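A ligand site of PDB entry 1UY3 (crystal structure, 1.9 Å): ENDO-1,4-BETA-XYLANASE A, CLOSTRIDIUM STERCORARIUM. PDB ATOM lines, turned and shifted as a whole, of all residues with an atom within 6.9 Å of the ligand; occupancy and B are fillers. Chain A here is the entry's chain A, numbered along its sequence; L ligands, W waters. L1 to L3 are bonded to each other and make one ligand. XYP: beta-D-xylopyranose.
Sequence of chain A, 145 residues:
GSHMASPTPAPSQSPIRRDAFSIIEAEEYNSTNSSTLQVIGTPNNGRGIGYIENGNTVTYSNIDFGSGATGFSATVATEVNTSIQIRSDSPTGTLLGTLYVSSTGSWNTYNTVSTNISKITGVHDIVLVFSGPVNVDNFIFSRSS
Water W2 bridges an oxygen (O2) of XYP L3 and the backbone NH of Gly 41.
Water W4 lies within hydrogen-bond range of an oxygen (O2) of XYP L1 (2.6 Å), the backbone carbonyl oxygen (O) of Val 134 (2.8 Å), the backbone NH (N) of Ile 52 (3.0 Å) and the backbone NH (N) of Tyr 51 (3.2 Å).
Water W1 lies within hydrogen-bond range of an oxygen (O3) of XYP L3 (2.6 Å), the backbone carbonyl oxygen of Thr 42 (3.1 Å) and the side-chain amide oxygen of Asn 45 (3.1 Å).
Water W3 bridges O of Ile 52 (2.8 Å) and O2 of XYP L1 (2.8 Å).
The side-chain amide nitrogen (ND2) of Asn 135 lies within hydrogen-bond range of the backbone carbonyl oxygen (O) of Trp 107, 2.9 Å away.
N of Asn 135 lies within hydrogen-bond range of O of Ala 77 (2.8 Å).
The side-chain hydroxyl of Thr 42 sits at hydrogen-bond distance from the backbone NH of Gly 46.
O of Gln 38 sits at hydrogen-bond distance from N of Gly 50 (3.0 Å).
The backbone NH (N) of Trp 107 lies close to the side-chain carboxylate (OE1) of Glu 79, 3.4 Å away.
OD1 of Asn 135 lies within hydrogen-bond range of O3 of XYP L1, 2.5 Å away.
N of Tyr 51 sits at hydrogen-bond distance from O3 of XYP L1 (2.9 Å).
The side-chain amide oxygen (OD1) of Asn 108 sits at hydrogen-bond distance from an oxygen (O3) of XYP L2 (3.0 Å).
The backbone carbonyl oxygen (O) of Thr 42 is in hydrogen-bond range of an oxygen (O4) of XYP L3, at 3.1 Å.
Merely in contact with the ligand: Pro 43 (3.4 Å), Gly 41 (3.5 Å), Gly 50 (3.5 Å), Trp 107 (3.5 Å), Pro 133 (3.6 Å) and Ile 40 (3.8 Å).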
ATOM      1  N   GLN A  38      -8.829  35.632   8.439  1.00  0.00           N
ATOM      2  CA  GLN A  38      -7.678  36.194   9.132  1.00  0.00           C
ATOM      3  C   GLN A  38      -6.441  35.345   8.941  1.00  0.00           C
ATOM      4  O   GLN A  38      -6.509  34.122   8.732  1.00  0.00           O
ATOM      5  CB  GLN A  38      -7.956  36.303  10.625  1.00  0.00           C
ATOM      6  CG  GLN A  38      -9.210  37.162  10.961  1.00  0.00           C
ATOM      7  CD  GLN A  38      -9.403  37.387  12.452  1.00  0.00           C
ATOM      8  OE1 GLN A  38      -8.426  37.305  13.215  1.00  0.00           O
ATOM      9  NE2 GLN A  38     -10.652  37.653  12.878  1.00  0.00           N
ATOM     10  N   ILE A  40      -3.794  33.569  10.867  1.00  0.00           N
ATOM     11  CA  ILE A  40      -3.760  32.986  12.207  1.00  0.00           C
ATOM     12  C   ILE A  40      -2.335  32.435  12.495  1.00  0.00           C
ATOM     13  O   ILE A  40      -1.547  32.215  11.591  1.00  0.00           O
ATOM     14  CB  ILE A  40      -4.831  31.889  12.344  1.00  0.00           C
ATOM     15  CG1 ILE A  40      -4.676  30.791  11.286  1.00  0.00           C
ATOM     16  CG2 ILE A  40      -6.226  32.529  12.266  1.00  0.00           C
ATOM     17  CD1 ILE A  40      -5.279  29.544  11.630  1.00  0.00           C
ATOM     18  N   GLY A  41      -2.035  32.222  13.763  1.00  0.00           N
ATOM     19  CA  GLY A  41      -0.838  31.497  14.161  1.00  0.00           C
ATOM     20  C   GLY A  41      -1.138  30.017  14.308  1.00  0.00           C
ATOM     21  O   GLY A  41      -2.283  29.600  14.458  1.00  0.00           O
ATOM     22  N   THR A  42      -0.065  29.219  14.316  1.00  0.00           N
ATOM     23  CA  THR A  42      -0.179  27.782  14.525  1.00  0.00           C
ATOM     24  C   THR A  42       0.629  27.399  15.748  1.00  0.00           C
ATOM     25  O   THR A  42       1.398  28.208  16.240  1.00  0.00           O
ATOM     26  CB  THR A  42       0.352  26.978  13.305  1.00  0.00           C
ATOM     27  OG1 THR A  42       1.761  27.226  13.144  1.00  0.00           O
ATOM     28  CG2 THR A  42      -0.327  27.423  11.987  1.00  0.00           C
ATOM     29  N   PRO A  43       0.397  26.198  16.294  1.00  0.00           N
ATOM     30  CA  PRO A  43       1.102  25.781  17.517  1.00  0.00           C
ATOM     31  C   PRO A  43       2.615  25.878  17.509  1.00  0.00           C
ATOM     32  O   PRO A  43       3.175  26.087  18.602  1.00  0.00           O
ATOM     33  CB  PRO A  43       0.617  24.348  17.722  1.00  0.00           C
ATOM     34  CG  PRO A  43      -0.750  24.402  17.136  1.00  0.00           C
ATOM     35  CD  PRO A  43      -0.644  25.223  15.923  1.00  0.00           C
ATOM     36  N   ASN A  44       3.276  25.716  16.367  1.00  0.00           N
ATOM     37  CA  ASN A  44       4.729  25.786  16.299  1.00  0.00           C
ATOM     38  C   ASN A  44       5.189  27.145  15.796  1.00  0.00           C
ATOM     39  O   ASN A  44       6.284  27.297  15.251  1.00  0.00           O
ATOM     40  CB  ASN A  44       5.328  24.607  15.440  1.00  0.00           C
ATOM     41  CG  ASN A  44       5.172  23.258  16.123  1.00  0.00           C
ATOM     42  OD1 ASN A  44       5.000  23.222  17.339  1.00  0.00           O
ATOM     43  ND2 ASN A  44       5.273  22.180  15.389  1.00  0.00           N
ATOM     44  N   ASN A  45       4.345  28.149  16.017  1.00  0.00           N
ATOM     45  CA  ASN A  45       4.636  29.543  15.696  1.00  0.00           C
ATOM     46  C   ASN A  45       4.809  29.801  14.206  1.00  0.00           C
ATOM     47  O   ASN A  45       5.546  30.669  13.775  1.00  0.00           O
ATOM     48  CB  ASN A  45       5.810  30.026  16.533  1.00  0.00           C
ATOM     49  CG  ASN A  45       5.442  30.062  18.000  1.00  0.00           C
ATOM     50  OD1 ASN A  45       4.378  30.609  18.372  1.00  0.00           O
ATOM     51  ND2 ASN A  45       6.269  29.431  18.856  1.00  0.00           N
ATOM     52  N   GLY A  46       4.086  29.028  13.403  1.00  0.00           N
ATOM     53  CA  GLY A  46       3.932  29.328  11.981  1.00  0.00           C
ATOM     54  C   GLY A  46       2.671  30.147  11.811  1.00  0.00           C
ATOM     55  O   GLY A  46       2.142  30.674  12.782  1.00  0.00           O
ATOM     56  N   ILE A  49      -4.211  30.530   7.377  1.00  0.00           N
ATOM     57  CA  ILE A  49      -5.422  31.243   7.219  1.00  0.00           C
ATOM     58  C   ILE A  49      -6.514  30.513   7.939  1.00  0.00           C
ATOM     59  O   ILE A  49      -6.541  29.286   7.970  1.00  0.00           O
ATOM     60  CB  ILE A  49      -5.787  31.519   5.736  1.00  0.00           C
ATOM     61  CG1 ILE A  49      -5.853  30.189   4.938  1.00  0.00           C
ATOM     62  CG2 ILE A  49      -4.800  32.455   5.148  1.00  0.00           C
ATOM     63  CD1 ILE A  49      -6.399  30.274   3.528  1.00  0.00           C
ATOM     64  N   GLY A  50      -7.396  31.297   8.558  1.00  0.00           N
ATOM     65  CA  GLY A  50      -8.560  30.794   9.221  1.00  0.00           C
ATOM     66  C   GLY A  50      -9.698  31.810   9.196  1.00  0.00           C
ATOM     67  O   GLY A  50      -9.660  32.757   8.423  1.00  0.00           O
ATOM     68  N   TYR A  51     -10.682  31.614  10.063  1.00  0.00           N
ATOM     69  CA  TYR A  51     -11.936  32.376  10.117  1.00  0.00           C
ATOM     70  C   TYR A  51     -12.604  32.405   8.748  1.00  0.00           C
ATOM     71  O   TYR A  51     -13.062  33.427   8.285  1.00  0.00           O
ATOM     72  CB  TYR A  51     -11.753  33.744  10.783  1.00  0.00           C
ATOM     73  CG  TYR A  51     -11.345  33.571  12.206  1.00  0.00           C
ATOM     74  CD1 TYR A  51     -10.011  33.502  12.552  1.00  0.00           C
ATOM     75  CD2 TYR A  51     -12.297  33.398  13.237  1.00  0.00           C
ATOM     76  CE1 TYR A  51      -9.606  33.302  13.888  1.00  0.00           C
ATOM     77  CE2 TYR A  51     -11.900  33.209  14.577  1.00  0.00           C
ATOM     78  CZ  TYR A  51     -10.562  33.162  14.894  1.00  0.00           C
ATOM     79  OH  TYR A  51     -10.170  32.947  16.219  1.00  0.00           O
ATOM     80  N   ILE A  52     -12.626  31.228   8.120  1.00  0.00           N
ATOM     81  CA  ILE A  52     -13.091  31.068   6.735  1.00  0.00           C
ATOM     82  C   ILE A  52     -14.538  30.624   6.755  1.00  0.00           C
ATOM     83  O   ILE A  52     -14.941  29.849   7.622  1.00  0.00           O
ATOM     84  CB  ILE A  52     -12.218  30.022   5.989  1.00  0.00           C
ATOM     85  CG1 ILE A  52     -10.885  30.646   5.577  1.00  0.00           C
ATOM     86  CG2 ILE A  52     -12.948  29.489   4.736  1.00  0.00           C
ATOM     87  CD1 ILE A  52      -9.850  29.610   5.241  1.00  0.00           C
ATOM     88  N   GLU A  53     -15.343  31.141   5.823  1.00  0.00           N
ATOM     89  CA  GLU A  53     -16.714  30.672   5.661  1.00  0.00           C
ATOM     90  C   GLU A  53     -16.993  30.119   4.293  1.00  0.00           C
ATOM     91  O   GLU A  53     -16.246  30.387   3.350  1.00  0.00           O
ATOM     92  CB  GLU A  53     -17.679  31.828   5.949  1.00  0.00           C
ATOM     93  CG  GLU A  53     -17.425  32.407   7.345  1.00  0.00           C
ATOM     94  CD  GLU A  53     -18.488  33.380   7.795  1.00  0.00           C
ATOM     95  OE1 GLU A  53     -19.005  34.102   6.932  1.00  0.00           O
ATOM     96  OE2 GLU A  53     -18.742  33.432   9.025  1.00  0.00           O
ATOM     97  N   ALA A  77      -6.315  22.008   9.475  1.00  0.00           N
ATOM     98  CA  ALA A  77      -6.935  21.631  10.767  1.00  0.00           C
ATOM     99  C   ALA A  77      -8.385  22.089  10.735  1.00  0.00           C
ATOM    100  O   ALA A  77      -8.684  23.200  10.326  1.00  0.00           O
ATOM    101  CB  ALA A  77      -6.241  22.336  11.908  1.00  0.00           C
ATOM    102  N   GLU A  79     -12.509  21.213  12.823  1.00  0.00           N
ATOM    103  CA  GLU A  79     -13.406  20.457  13.686  1.00  0.00           C
ATOM    104  C   GLU A  79     -14.674  19.976  12.999  1.00  0.00           C
ATOM    105  O   GLU A  79     -15.502  19.305  13.595  1.00  0.00           O
ATOM    106  CB  GLU A  79     -13.704  21.282  14.946  1.00  0.00           C
ATOM    107  CG  GLU A  79     -12.458  21.431  15.799  1.00  0.00           C
ATOM    108  CD  GLU A  79     -12.727  21.746  17.237  1.00  0.00           C
ATOM    109  OE1 GLU A  79     -11.750  21.993  17.974  1.00  0.00           O
ATOM    110  OE2 GLU A  79     -13.911  21.791  17.638  1.00  0.00           O
ATOM    111  N   TRP A 107      -9.001  22.748  16.032  1.00  0.00           N
ATOM    112  CA  TRP A 107      -8.592  23.856  15.145  1.00  0.00           C
ATOM    113  C   TRP A 107      -7.084  23.996  15.110  1.00  0.00           C
ATOM    114  O   TRP A 107      -6.550  24.695  14.248  1.00  0.00           O
ATOM    115  CB  TRP A 107      -9.235  25.165  15.623  1.00  0.00           C
ATOM    116  CG  TRP A 107     -10.746  25.107  15.552  1.00  0.00           C
ATOM    117  CD1 TRP A 107     -11.627  25.105  16.630  1.00  0.00           C
ATOM    118  CD2 TRP A 107     -11.552  24.991  14.383  1.00  0.00           C
ATOM    119  NE1 TRP A 107     -12.918  25.011  16.180  1.00  0.00           N
ATOM    120  CE2 TRP A 107     -12.918  24.947  14.810  1.00  0.00           C
ATOM    121  CE3 TRP A 107     -11.294  24.971  13.017  1.00  0.00           C
ATOM    122  CZ2 TRP A 107     -13.995  24.873  13.890  1.00  0.00           C
ATOM    123  CZ3 TRP A 107     -12.333  24.879  12.127  1.00  0.00           C
ATOM    124  CH2 TRP A 107     -13.669  24.826  12.543  1.00  0.00           C
ATOM    125  N   ASN A 108      -6.404  23.340  16.048  1.00  0.00           N
ATOM    126  CA  ASN A 108      -4.948  23.381  16.122  1.00  0.00           C
ATOM    127  C   ASN A 108      -4.231  22.044  15.863  1.00  0.00           C
ATOM    128  O   ASN A 108      -3.049  21.938  16.051  1.00  0.00           O
ATOM    129  CB  ASN A 108      -4.526  23.981  17.445  1.00  0.00           C
ATOM    130  CG  ASN A 108      -5.067  25.396  17.643  1.00  0.00           C
ATOM    131  OD1 ASN A 108      -5.827  25.669  18.570  1.00  0.00           O
ATOM    132  ND2 ASN A 108      -4.659  26.298  16.774  1.00  0.00           N
ATOM    133  N   TYR A 110      -3.165  19.971  13.077  1.00  0.00           N
ATOM    134  CA  TYR A 110      -2.932  19.929  11.614  1.00  0.00           C
ATOM    135  C   TYR A 110      -2.606  18.539  11.073  1.00  0.00           C
ATOM    136  O   TYR A 110      -2.026  17.726  11.752  1.00  0.00           O
ATOM    137  CB  TYR A 110      -1.872  20.952  11.240  1.00  0.00           C
ATOM    138  CG  TYR A 110      -2.383  22.359  11.368  1.00  0.00           C
ATOM    139  CD1 TYR A 110      -2.434  22.982  12.619  1.00  0.00           C
ATOM    140  CD2 TYR A 110      -2.923  23.036  10.266  1.00  0.00           C
ATOM    141  CE1 TYR A 110      -2.938  24.273  12.775  1.00  0.00           C
ATOM    142  CE2 TYR A 110      -3.459  24.362  10.410  1.00  0.00           C
ATOM    143  CZ  TYR A 110      -3.464  24.961  11.671  1.00  0.00           C
ATOM    144  OH  TYR A 110      -3.945  26.240  11.883  1.00  0.00           O
ATOM    145  N   GLY A 132     -16.776  25.662   3.974  1.00  0.00           N
ATOM    146  CA  GLY A 132     -16.899  25.788   5.425  1.00  0.00           C
ATOM    147  C   GLY A 132     -15.548  26.071   6.086  1.00  0.00           C
ATOM    148  O   GLY A 132     -14.487  26.158   5.381  1.00  0.00           O
ATOM    149  N   PRO A 133     -15.595  26.223   7.420  1.00  0.00           N
ATOM    150  CA  PRO A 133     -14.409  26.556   8.208  1.00  0.00           C
ATOM    151  C   PRO A 133     -13.310  25.459   8.159  1.00  0.00           C
ATOM    152  O   PRO A 133     -13.600  24.285   8.236  1.00  0.00           O
ATOM    153  CB  PRO A 133     -14.950  26.718   9.643  1.00  0.00           C
ATOM    154  CG  PRO A 133     -16.196  25.994   9.660  1.00  0.00           C
ATOM    155  CD  PRO A 133     -16.785  26.072   8.279  1.00  0.00           C
ATOM    156  N   VAL A 134     -12.073  25.926   7.998  1.00  0.00           N
ATOM    157  CA  VAL A 134     -10.873  25.090   8.001  1.00  0.00           C
ATOM    158  C   VAL A 134      -9.716  26.060   8.201  1.00  0.00           C
ATOM    159  O   VAL A 134      -9.752  27.177   7.736  1.00  0.00           O
ATOM    160  CB  VAL A 134     -10.758  24.252   6.707  1.00  0.00           C
ATOM    161  CG1 VAL A 134     -10.854  25.139   5.487  1.00  0.00           C
ATOM    162  CG2 VAL A 134      -9.463  23.395   6.668  1.00  0.00           C
ATOM    163  N   ASN A 135      -8.687  25.628   8.902  1.00  0.00           N
ATOM    164  CA  ASN A 135      -7.469  26.349   8.989  1.00  0.00           C
ATOM    165  C   ASN A 135      -6.462  25.716   8.020  1.00  0.00           C
ATOM    166  O   ASN A 135      -6.301  24.478   7.973  1.00  0.00           O
ATOM    167  CB  ASN A 135      -6.964  26.312  10.435  1.00  0.00           C
ATOM    168  CG  ASN A 135      -7.822  27.118  11.388  1.00  0.00           C
ATOM    169  OD1 ASN A 135      -8.548  28.004  10.940  1.00  0.00           O
ATOM    170  ND2 ASN A 135      -7.722  26.850  12.731  1.00  0.00           N
HETATM  171  O1  XYP L   1     -14.656  28.974  13.890  1.00  0.00           O
HETATM  172  C1  XYP L   1     -13.272  28.692  13.940  1.00  0.00           C
HETATM  173  C2  XYP L   1     -12.425  29.349  12.846  1.00  0.00           C
HETATM  174  C3  XYP L   1     -10.977  28.953  13.045  1.00  0.00           C
HETATM  175  C4  XYP L   1     -10.494  29.245  14.471  1.00  0.00           C
HETATM  176  C5  XYP L   1     -11.478  28.661  15.448  1.00  0.00           C
HETATM  177  O2  XYP L   1     -12.837  28.942  11.562  1.00  0.00           O
HETATM  178  O3  XYP L   1     -10.101  29.597  12.134  1.00  0.00           O
HETATM  179  O4  XYP L   1      -9.202  28.683  14.676  1.00  0.00           O
HETATM  180  O5  XYP L   1     -12.797  29.108  15.159  1.00  0.00           O
HETATM  181  C1  XYP L   2      -8.365  29.453  15.559  1.00  0.00           C
HETATM  182  C2  XYP L   2      -8.087  28.586  16.766  1.00  0.00           C
HETATM  183  C3  XYP L   2      -7.132  29.270  17.732  1.00  0.00           C
HETATM  184  C4  XYP L   2      -5.866  29.599  16.971  1.00  0.00           C
HETATM  185  C5  XYP L   2      -6.178  30.397  15.724  1.00  0.00           C
HETATM  186  O2  XYP L   2      -9.320  28.235  17.373  1.00  0.00           O
HETATM  187  O3  XYP L   2      -6.836  28.434  18.864  1.00  0.00           O
HETATM  188  O4  XYP L   2      -4.974  30.335  17.756  1.00  0.00           O
HETATM  189  O5  XYP L   2      -7.189  29.752  14.944  1.00  0.00           O
HETATM  190  C1  XYP L   3      -3.594  29.870  17.654  1.00  0.00           C
HETATM  191  C2  XYP L   3      -2.679  30.925  18.232  1.00  0.00           C
HETATM  192  C3  XYP L   3      -1.235  30.410  18.149  1.00  0.00           C
HETATM  193  C4  XYP L   3      -1.196  29.093  18.889  1.00  0.00           C
HETATM  194  C5  XYP L   3      -2.049  28.112  18.114  1.00  0.00           C
HETATM  195  O2  XYP L   3      -2.811  32.187  17.593  1.00  0.00           O
HETATM  196  O3  XYP L   3      -0.321  31.310  18.737  1.00  0.00           O
HETATM  197  O4  XYP L   3       0.127  28.675  19.000  1.00  0.00           O
HETATM  198  O5  XYP L   3      -3.378  28.627  18.218  1.00  0.00           O
HETATM  199  O   HOH W   1       1.655  31.142  17.063  1.00  0.00           O
HETATM  200  O   HOH W   2      -4.176  32.766  15.701  1.00  0.00           O
HETATM  201  O   HOH W   3     -14.842  30.480  10.342  1.00  0.00           O
HETATM  202  O   HOH W   4     -11.620  28.651   9.292  1.00  0.00           O
